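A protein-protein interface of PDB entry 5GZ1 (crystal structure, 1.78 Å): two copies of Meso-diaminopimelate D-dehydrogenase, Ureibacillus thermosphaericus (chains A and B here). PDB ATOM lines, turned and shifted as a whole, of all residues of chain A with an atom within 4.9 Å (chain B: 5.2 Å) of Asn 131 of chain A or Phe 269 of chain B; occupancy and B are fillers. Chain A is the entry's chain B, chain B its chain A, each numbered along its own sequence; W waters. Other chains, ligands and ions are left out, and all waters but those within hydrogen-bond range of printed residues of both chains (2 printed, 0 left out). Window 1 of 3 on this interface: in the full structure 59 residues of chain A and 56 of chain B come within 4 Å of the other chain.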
ATOM      1  N   LEU A 127      21.111  29.312  16.386  1.00  0.00           N
ATOM      2  CA  LEU A 127      19.720  28.958  16.175  1.00  0.00           C
ATOM      3  C   LEU A 127      18.783  30.117  16.567  1.00  0.00           C
ATOM      4  O   LEU A 127      17.790  30.363  15.886  1.00  0.00           O
ATOM      5  CB  LEU A 127      19.369  27.746  16.972  1.00  0.00           C
ATOM      6  CG  LEU A 127      20.159  26.454  16.770  1.00  0.00           C
ATOM      7  CD1 LEU A 127      19.373  25.300  17.411  1.00  0.00           C
ATOM      8  CD2 LEU A 127      20.508  26.158  15.343  1.00  0.00           C
ATOM      9  N   PHE A 128      19.115  30.881  17.650  1.00  0.00           N
ATOM     10  CA  PHE A 128      18.249  32.057  17.955  1.00  0.00           C
ATOM     11  C   PHE A 128      18.342  33.111  16.889  1.00  0.00           C
ATOM     12  O   PHE A 128      17.322  33.728  16.564  1.00  0.00           O
ATOM     13  CB  PHE A 128      18.603  32.627  19.322  1.00  0.00           C
ATOM     14  CG  PHE A 128      17.980  31.930  20.496  1.00  0.00           C
ATOM     15  CD1 PHE A 128      17.415  30.639  20.432  1.00  0.00           C
ATOM     16  CD2 PHE A 128      18.041  32.528  21.733  1.00  0.00           C
ATOM     17  CE1 PHE A 128      16.789  30.049  21.501  1.00  0.00           C
ATOM     18  CE2 PHE A 128      17.487  31.897  22.831  1.00  0.00           C
ATOM     19  CZ  PHE A 128      16.858  30.657  22.724  1.00  0.00           C
ATOM     20  N   SER A 129      19.506  33.303  16.288  1.00  0.00           N
ATOM     21  CA  SER A 129      19.654  34.245  15.211  1.00  0.00           C
ATOM     22  C   SER A 129      18.816  33.906  14.035  1.00  0.00           C
ATOM     23  O   SER A 129      18.125  34.737  13.455  1.00  0.00           O
ATOM     24  CB  SER A 129      21.116  34.278  14.807  1.00  0.00           C
ATOM     25  OG  SER A 129      21.991  34.342  15.937  1.00  0.00           O
ATOM     26  N   LEU A 130      18.817  32.605  13.682  1.00  0.00           N
ATOM     27  CA  LEU A 130      17.998  32.110  12.581  1.00  0.00           C
ATOM     28  C   LEU A 130      16.582  32.433  12.841  1.00  0.00           C
ATOM     29  O   LEU A 130      15.851  32.753  11.941  1.00  0.00           O
ATOM     30  CB  LEU A 130      18.175  30.571  12.384  1.00  0.00           C
ATOM     31  CG  LEU A 130      19.511  30.232  11.773  1.00  0.00           C
ATOM     32  CD1 LEU A 130      19.773  28.772  12.010  1.00  0.00           C
ATOM     33  CD2 LEU A 130      19.475  30.534  10.291  1.00  0.00           C
ATOM     34  N   ASN A 131      16.105  32.203  14.079  1.00  0.00           N
ATOM     35  CA  ASN A 131      14.696  32.375  14.343  1.00  0.00           C
ATOM     36  C   ASN A 131      14.343  33.858  14.415  1.00  0.00           C
ATOM     37  O   ASN A 131      13.180  34.200  14.056  1.00  0.00           O
ATOM     38  CB  ASN A 131      14.296  31.645  15.569  1.00  0.00           C
ATOM     39  CG  ASN A 131      14.007  30.209  15.243  1.00  0.00           C
ATOM     40  OD1 ASN A 131      12.891  29.889  14.792  1.00  0.00           O
ATOM     41  ND2 ASN A 131      15.032  29.387  15.257  1.00  0.00           N
ATOM     42  N   ARG A 132      15.270  34.699  14.916  1.00  0.00           N
ATOM     43  CA  ARG A 132      15.033  36.178  14.804  1.00  0.00           C
ATOM     44  C   ARG A 132      14.799  36.563  13.324  1.00  0.00           C
ATOM     45  O   ARG A 132      13.897  37.300  13.010  1.00  0.00           O
ATOM     46  CB  ARG A 132      16.138  37.048  15.418  1.00  0.00           C
ATOM     47  CG  ARG A 132      16.090  37.013  16.951  1.00  0.00           C
ATOM     48  CD  ARG A 132      17.136  37.950  17.517  1.00  0.00           C
ATOM     49  NE  ARG A 132      18.519  37.526  17.440  1.00  0.00           N
ATOM     50  CZ  ARG A 132      19.164  36.786  18.307  1.00  0.00           C
ATOM     51  NH1 ARG A 132      20.415  36.527  18.104  1.00  0.00           N
ATOM     52  NH2 ARG A 132      18.604  36.349  19.445  1.00  0.00           N
ATOM     53  N   LEU A 133      15.652  36.056  12.450  1.00  0.00           N
ATOM     54  CA  LEU A 133      15.574  36.385  11.052  1.00  0.00           C
ATOM     55  C   LEU A 133      14.255  35.863  10.399  1.00  0.00           C
ATOM     56  O   LEU A 133      13.537  36.592   9.721  1.00  0.00           O
ATOM     57  CB  LEU A 133      16.820  35.872  10.304  1.00  0.00           C
ATOM     58  CG  LEU A 133      16.852  36.104   8.801  1.00  0.00           C
ATOM     59  CD1 LEU A 133      16.575  37.522   8.523  1.00  0.00           C
ATOM     60  CD2 LEU A 133      18.226  35.714   8.214  1.00  0.00           C
ATOM     61  N   LEU A 134      13.959  34.579  10.628  1.00  0.00           N
ATOM     62  CA  LEU A 134      12.786  33.970  10.088  1.00  0.00           C
ATOM     63  C   LEU A 134      11.581  34.769  10.524  1.00  0.00           C
ATOM     64  O   LEU A 134      10.666  35.044   9.743  1.00  0.00           O
ATOM     65  CB  LEU A 134      12.675  32.509  10.585  1.00  0.00           C
ATOM     66  CG  LEU A 134      11.484  31.777  10.020  1.00  0.00           C
ATOM     67  CD1 LEU A 134      11.751  31.662   8.515  1.00  0.00           C
ATOM     68  CD2 LEU A 134      11.441  30.406  10.686  1.00  0.00           C
ATOM     69  N   GLY A 135      11.528  35.166  11.797  1.00  0.00           N
ATOM     70  CA  GLY A 135      10.389  35.942  12.227  1.00  0.00           C
ATOM     71  C   GLY A 135      10.179  37.213  11.489  1.00  0.00           C
ATOM     72  O   GLY A 135       9.034  37.569  11.116  1.00  0.00           O
ATOM     73  N   VAL A 253      12.768  32.832  21.510  1.00  0.00           N
ATOM     74  CA  VAL A 253      12.670  33.895  20.546  1.00  0.00           C
ATOM     75  C   VAL A 253      11.270  33.919  20.068  1.00  0.00           C
ATOM     76  O   VAL A 253      10.707  32.891  19.603  1.00  0.00           O
ATOM     77  CB  VAL A 253      13.605  33.663  19.317  1.00  0.00           C
ATOM     78  CG1 VAL A 253      13.420  34.775  18.325  1.00  0.00           C
ATOM     79  CG2 VAL A 253      15.043  33.656  19.798  1.00  0.00           C
ATOM     80  N   ILE A 267       4.946  33.591  16.341  1.00  0.00           N
ATOM     81  CA  ILE A 267       5.932  32.542  16.111  1.00  0.00           C
ATOM     82  C   ILE A 267       6.814  32.467  17.332  1.00  0.00           C
ATOM     83  O   ILE A 267       7.352  33.482  17.834  1.00  0.00           O
ATOM     84  CB  ILE A 267       6.862  32.870  14.902  1.00  0.00           C
ATOM     85  CG1 ILE A 267       6.100  33.135  13.613  1.00  0.00           C
ATOM     86  CG2 ILE A 267       7.879  31.773  14.708  1.00  0.00           C
ATOM     87  CD1 ILE A 267       6.979  33.761  12.550  1.00  0.00           C
ATOM     88  N   GLU A 268       7.025  31.269  17.849  1.00  0.00           N
ATOM     89  CA  GLU A 268       7.894  31.066  19.009  1.00  0.00           C
ATOM     90  C   GLU A 268       8.859  29.892  18.837  1.00  0.00           C
ATOM     91  O   GLU A 268       8.505  28.865  18.398  1.00  0.00           O
ATOM     92  CB  GLU A 268       7.098  30.811  20.283  1.00  0.00           C
ATOM     93  CG  GLU A 268       7.903  30.755  21.575  1.00  0.00           C
ATOM     94  CD  GLU A 268       7.019  30.607  22.822  1.00  0.00           C
ATOM     95  OE1 GLU A 268       5.916  31.154  22.853  1.00  0.00           O
ATOM     96  OE2 GLU A 268       7.419  29.912  23.756  1.00  0.00           O
ATOM     97  N   PHE A 269      10.073  30.135  19.238  1.00  0.00           N
ATOM     98  CA  PHE A 269      11.159  29.128  19.234  1.00  0.00           C
ATOM     99  C   PHE A 269      11.749  29.042  20.569  1.00  0.00           C
ATOM    100  O   PHE A 269      12.049  30.091  21.190  1.00  0.00           O
ATOM    101  CB  PHE A 269      12.236  29.467  18.171  1.00  0.00           C
ATOM    102  CG  PHE A 269      13.394  28.462  18.109  1.00  0.00           C
ATOM    103  CD1 PHE A 269      13.238  27.240  17.393  1.00  0.00           C
ATOM    104  CD2 PHE A 269      14.592  28.683  18.744  1.00  0.00           C
ATOM    105  CE1 PHE A 269      14.307  26.372  17.276  1.00  0.00           C
ATOM    106  CE2 PHE A 269      15.655  27.797  18.623  1.00  0.00           C
ATOM    107  CZ  PHE A 269      15.484  26.613  17.930  1.00  0.00           C
ATOM    108  N   LEU B 127       7.813  25.912   7.209  1.00  0.00           N
ATOM    109  CA  LEU B 127       8.475  26.281   8.422  1.00  0.00           C
ATOM    110  C   LEU B 127       8.587  25.070   9.410  1.00  0.00           C
ATOM    111  O   LEU B 127       9.617  24.802  10.011  1.00  0.00           O
ATOM    112  CB  LEU B 127       7.849  27.432   9.162  1.00  0.00           C
ATOM    113  CG  LEU B 127       7.712  28.753   8.369  1.00  0.00           C
ATOM    114  CD1 LEU B 127       7.387  29.824   9.383  1.00  0.00           C
ATOM    115  CD2 LEU B 127       8.941  29.062   7.610  1.00  0.00           C
ATOM    116  N   PHE B 128       7.518  24.298   9.515  1.00  0.00           N
ATOM    117  CA  PHE B 128       7.564  23.086  10.313  1.00  0.00           C
ATOM    118  C   PHE B 128       8.593  22.063   9.785  1.00  0.00           C
ATOM    119  O   PHE B 128       9.256  21.470  10.550  1.00  0.00           O
ATOM    120  CB  PHE B 128       6.191  22.427  10.449  1.00  0.00           C
ATOM    121  CG  PHE B 128       5.324  23.017  11.507  1.00  0.00           C
ATOM    122  CD1 PHE B 128       5.628  24.204  12.085  1.00  0.00           C
ATOM    123  CD2 PHE B 128       4.178  22.375  11.893  1.00  0.00           C
ATOM    124  CE1 PHE B 128       4.834  24.719  13.043  1.00  0.00           C
ATOM    125  CE2 PHE B 128       3.365  22.900  12.833  1.00  0.00           C
ATOM    126  CZ  PHE B 128       3.695  24.074  13.407  1.00  0.00           C
ATOM    127  N   ASN B 131      11.949  22.991  10.813  1.00  0.00           N
ATOM    128  CA  ASN B 131      12.167  22.715  12.239  1.00  0.00           C
ATOM    129  C   ASN B 131      12.364  21.263  12.519  1.00  0.00           C
ATOM    130  O   ASN B 131      13.153  20.891  13.412  1.00  0.00           O
ATOM    131  CB  ASN B 131      11.157  23.427  13.133  1.00  0.00           C
ATOM    132  CG  ASN B 131      11.569  24.888  13.346  1.00  0.00           C
ATOM    133  OD1 ASN B 131      12.382  25.219  14.222  1.00  0.00           O
ATOM    134  ND2 ASN B 131      11.115  25.763  12.425  1.00  0.00           N
ATOM    135  N   LEU B 134      16.070  20.780  11.461  1.00  0.00           N
ATOM    136  CA  LEU B 134      16.963  21.317  12.393  1.00  0.00           C
ATOM    137  C   LEU B 134      17.098  20.484  13.628  1.00  0.00           C
ATOM    138  O   LEU B 134      18.174  20.251  14.143  1.00  0.00           O
ATOM    139  CB  LEU B 134      16.484  22.695  12.787  1.00  0.00           C
ATOM    140  CG  LEU B 134      17.393  23.537  13.611  1.00  0.00           C
ATOM    141  CD1 LEU B 134      18.607  23.776  12.728  1.00  0.00           C
ATOM    142  CD2 LEU B 134      16.661  24.871  13.963  1.00  0.00           C
ATOM    143  N   GLY B 251       0.272  25.205  15.814  1.00  0.00           N
ATOM    144  CA  GLY B 251       0.891  23.936  16.094  1.00  0.00           C
ATOM    145  C   GLY B 251       2.273  24.032  16.686  1.00  0.00           C
ATOM    146  O   GLY B 251       2.755  25.129  17.020  1.00  0.00           O
ATOM    147  N   PHE B 252       2.885  22.867  16.736  1.00  0.00           N
ATOM    148  CA  PHE B 252       4.118  22.626  17.458  1.00  0.00           C
ATOM    149  C   PHE B 252       4.929  21.609  16.731  1.00  0.00           C
ATOM    150  O   PHE B 252       4.386  20.570  16.275  1.00  0.00           O
ATOM    151  CB  PHE B 252       3.856  21.937  18.879  1.00  0.00           C
ATOM    152  CG  PHE B 252       3.032  22.710  19.785  1.00  0.00           C
ATOM    153  CD1 PHE B 252       3.551  23.777  20.441  1.00  0.00           C
ATOM    154  CD2 PHE B 252       1.678  22.399  19.927  1.00  0.00           C
ATOM    155  CE1 PHE B 252       2.750  24.546  21.274  1.00  0.00           C
ATOM    156  CE2 PHE B 252       0.881  23.127  20.802  1.00  0.00           C
ATOM    157  CZ  PHE B 252       1.419  24.196  21.474  1.00  0.00           C
ATOM    158  N   VAL B 253       6.244  21.876  16.604  1.00  0.00           N
ATOM    159  CA  VAL B 253       7.238  20.884  16.268  1.00  0.00           C
ATOM    160  C   VAL B 253       8.194  20.816  17.446  1.00  0.00           C
ATOM    161  O   VAL B 253       8.816  21.809  17.853  1.00  0.00           O
ATOM    162  CB  VAL B 253       8.012  21.195  14.925  1.00  0.00           C
ATOM    163  CG1 VAL B 253       9.089  20.178  14.684  1.00  0.00           C
ATOM    164  CG2 VAL B 253       7.065  21.216  13.802  1.00  0.00           C
ATOM    165  N   ILE B 254       8.341  19.581  18.021  1.00  0.00           N
ATOM    166  CA  ILE B 254       9.196  19.428  19.147  1.00  0.00           C
ATOM    167  C   ILE B 254      10.200  18.332  18.857  1.00  0.00           C
ATOM    168  O   ILE B 254       9.810  17.219  18.392  1.00  0.00           O
ATOM    169  CB  ILE B 254       8.410  19.123  20.449  1.00  0.00           C
ATOM    170  CG1 ILE B 254       7.515  20.287  20.851  1.00  0.00           C
ATOM    171  CG2 ILE B 254       9.349  18.829  21.611  1.00  0.00           C
ATOM    172  CD1 ILE B 254       6.471  19.961  21.892  1.00  0.00           C
ATOM    173  N   ILE B 267      13.990  21.056  21.868  1.00  0.00           N
ATOM    174  CA  ILE B 267      13.778  22.185  20.976  1.00  0.00           C
ATOM    175  C   ILE B 267      12.289  22.241  20.654  1.00  0.00           C
ATOM    176  O   ILE B 267      11.687  21.233  20.270  1.00  0.00           O
ATOM    177  CB  ILE B 267      14.569  21.976  19.671  1.00  0.00           C
ATOM    178  CG1 ILE B 267      16.024  21.690  19.910  1.00  0.00           C
ATOM    179  CG2 ILE B 267      14.367  23.160  18.733  1.00  0.00           C
ATOM    180  CD1 ILE B 267      16.831  21.259  18.693  1.00  0.00           C
ATOM    181  N   GLU B 268      11.702  23.430  20.705  1.00  0.00           N
ATOM    182  CA  GLU B 268      10.317  23.587  20.307  1.00  0.00           C
ATOM    183  C   GLU B 268      10.113  24.776  19.388  1.00  0.00           C
ATOM    184  O   GLU B 268      10.615  25.856  19.646  1.00  0.00           O
ATOM    185  CB  GLU B 268       9.453  23.633  21.568  1.00  0.00           C
ATOM    186  CG  GLU B 268       7.995  23.837  21.325  1.00  0.00           C
ATOM    187  CD  GLU B 268       7.140  23.785  22.632  1.00  0.00           C
ATOM    188  OE1 GLU B 268       7.504  23.133  23.676  1.00  0.00           O
ATOM    189  OE2 GLU B 268       6.066  24.424  22.590  1.00  0.00           O
ATOM    190  N   PHE B 269       9.340  24.600  18.359  1.00  0.00           N
ATOM    191  CA  PHE B 269       8.940  25.690  17.428  1.00  0.00           C
ATOM    192  C   PHE B 269       7.485  25.683  17.392  1.00  0.00           C
ATOM    193  O   PHE B 269       6.832  24.632  17.145  1.00  0.00           O
ATOM    194  CB  PHE B 269       9.473  25.419  16.041  1.00  0.00           C
ATOM    195  CG  PHE B 269       9.095  26.475  15.017  1.00  0.00           C
ATOM    196  CD1 PHE B 269       9.802  27.638  14.960  1.00  0.00           C
ATOM    197  CD2 PHE B 269       8.020  26.247  14.168  1.00  0.00           C
ATOM    198  CE1 PHE B 269       9.454  28.586  14.002  1.00  0.00           C
ATOM    199  CE2 PHE B 269       7.675  27.175  13.209  1.00  0.00           C
ATOM    200  CZ  PHE B 269       8.388  28.370  13.171  1.00  0.00           C
ATOM    201  N   SER B 270       6.858  26.839  17.602  1.00  0.00           N
ATOM    202  CA  SER B 270       5.381  26.882  17.629  1.00  0.00           C
ATOM    203  C   SER B 270       4.768  28.086  16.890  1.00  0.00           C
ATOM    204  O   SER B 270       5.441  29.116  16.737  1.00  0.00           O
ATOM    205  CB  SER B 270       4.821  26.920  19.064  1.00  0.00           C
ATOM    206  OG  SER B 270       5.160  28.036  19.735  1.00  0.00           O
ATOM    207  N   LEU B 271       3.559  27.867  16.376  1.00  0.00           N
ATOM    208  CA  LEU B 271       2.786  28.902  15.728  1.00  0.00           C
ATOM    209  C   LEU B 271       1.382  29.052  16.397  1.00  0.00           C
ATOM    210  O   LEU B 271       0.752  28.054  16.747  1.00  0.00           O
ATOM    211  CB  LEU B 271       2.630  28.622  14.246  1.00  0.00           C
ATOM    212  CG  LEU B 271       3.902  28.554  13.410  1.00  0.00           C
ATOM    213  CD1 LEU B 271       3.434  28.015  12.079  1.00  0.00           C
ATOM    214  CD2 LEU B 271       4.577  29.883  13.375  1.00  0.00           C
HETATM  215  O   HOH W   1       8.255  27.213  21.068  1.00  0.00           O
HETATM  216  O   HOH W   2      13.455  27.499  13.478  1.00  0.00           O
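Asn 131 of chain A touches Phe 269 of chain B, and with the chains exchanged Phe 269 of chain A touches Asn 131 of chain B.
Leu 134 of chain A touches Leu 127 of chain B, but with the chains exchanged Leu 127 of chain A does not touch Leu 134 of chain B (4.02 Å).
Ile 267 of chain A touches Phe 269 of chain B, and with the chains exchanged Phe 269 of chain A touches Ile 267 of chain B.
Glu 268 of chain A touches Phe 269 of chain B, and with the chains exchanged Phe 269 of chain A touches Glu 268 of chain B.
Of the 11 pairs that touch across the chains among the printed residues, 7 have their exchanged pair printed and touching as well.
The side-chain amide nitrogen (ND2) of Asn 131 of chain B sits at hydrogen-bond distance from the backbone carbonyl oxygen (O) of Leu 127 of chain B, 3.0 Å away.
The backbone carbonyl oxygen (O) of Gly 251 of chain B sits at hydrogen-bond distance from the backbone NH (N) of Leu 271 of chain B, at 2.9 Å.
The backbone carbonyl oxygen (O) of Phe 269 of chain B sits at hydrogen-bond distance from the backbone NH (N) of Val 253 of chain B (2.9 Å).
The side-chain amide nitrogen of Asn 131 of chain A lies within hydrogen-bond range of the backbone carbonyl oxygen of Leu 127 of chain A, at 3.0 Å.
The backbone carbonyl oxygen of Val 253 of chain A lies within hydrogen-bond range of the backbone NH of Phe 269 of chain A (2.9 Å).
The backbone NH (N) of Ser 270 of chain B is in hydrogen-bond range of the backbone carbonyl oxygen (O) of Glu 268 of chain A.
Water W2 lies within hydrogen-bond range of the side-chain amide oxygen of Asn 131 of chain B and the side-chain amide oxygen of Asn 131 of chain A.
Water W1 lies within hydrogen-bond range of O of Glu 268 of chain B, O of Glu 268 of chain A and OG of Ser 270 of chain B.
Of the 13 printed residues of chain B, 7 touch a printed residue of chain A.
Hydrophobic or aromatic side chains of chain B within 4 Å of the printed part of chain A: Leu 127, Ile 267, Phe 269 and Leu 271.
Of the 13 printed residues of chain A, 5 touch a printed residue of chain B.
Printed residues of chain A that touch a printed residue of chain B: Asn 131, Leu 134, Ile 267, Glu 268 and Phe 269.
Hydrophobic or aromatic side chains of chain A within 4 Å of the printed part of chain B: Leu 134, Ile 267 and Phe 269.
Among the printed residues, 11 pairs touch across the chains.
Among the printed residues, no Asp or Glu carboxylate lies within 4 Å of a Lys or Arg side-chain nitrogen of the other chain.
Among the printed residues, pairs that only touch across the chains: Phe 269 of chain A with Glu 268 of chain B, Glu 268 of chain A with Phe 269 of chain B, Ile 267 of chain A with Ser 270 of chain B, Phe 269 of chain A with Ile 267 of chain B, Ile 267 of chain A with Leu 271 of chain B, Ile 267 of chain A with Phe 269 of chain B, Asn 131 of chain A with Phe 269 of chain B, Phe 269 of chain A with Asn 131 of chain B, Glu 268 of chain A with Glu 268 of chain B and Leu 134 of chain A with Leu 127 of chain B.
Asn 131 of chain A touches just one residue of chain B: Phe 269.
Of the printed residues of chain B, Leu 134 of chain A touches Leu 127.
Of the printed residues of chain A, Leu 127 of chain B touches Leu 134.
Printed residues of chain A within 4 Å of Ile 267 of chain B: Phe 269.
Of chain A, only Asn 131 (3.8 Å), Ile 267 (3.6 Å) and Glu 268 (3.3 Å) come within 4 Å of Phe 269 of chain B.
The nearest residue of chain B that does not touch Asn 131 of chain A is Asn 131 of chain B (4.7 Å).
The nearest residue of chain A that does not touch Phe 269 of chain B is Phe 269 of chain A (4.2 Å).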
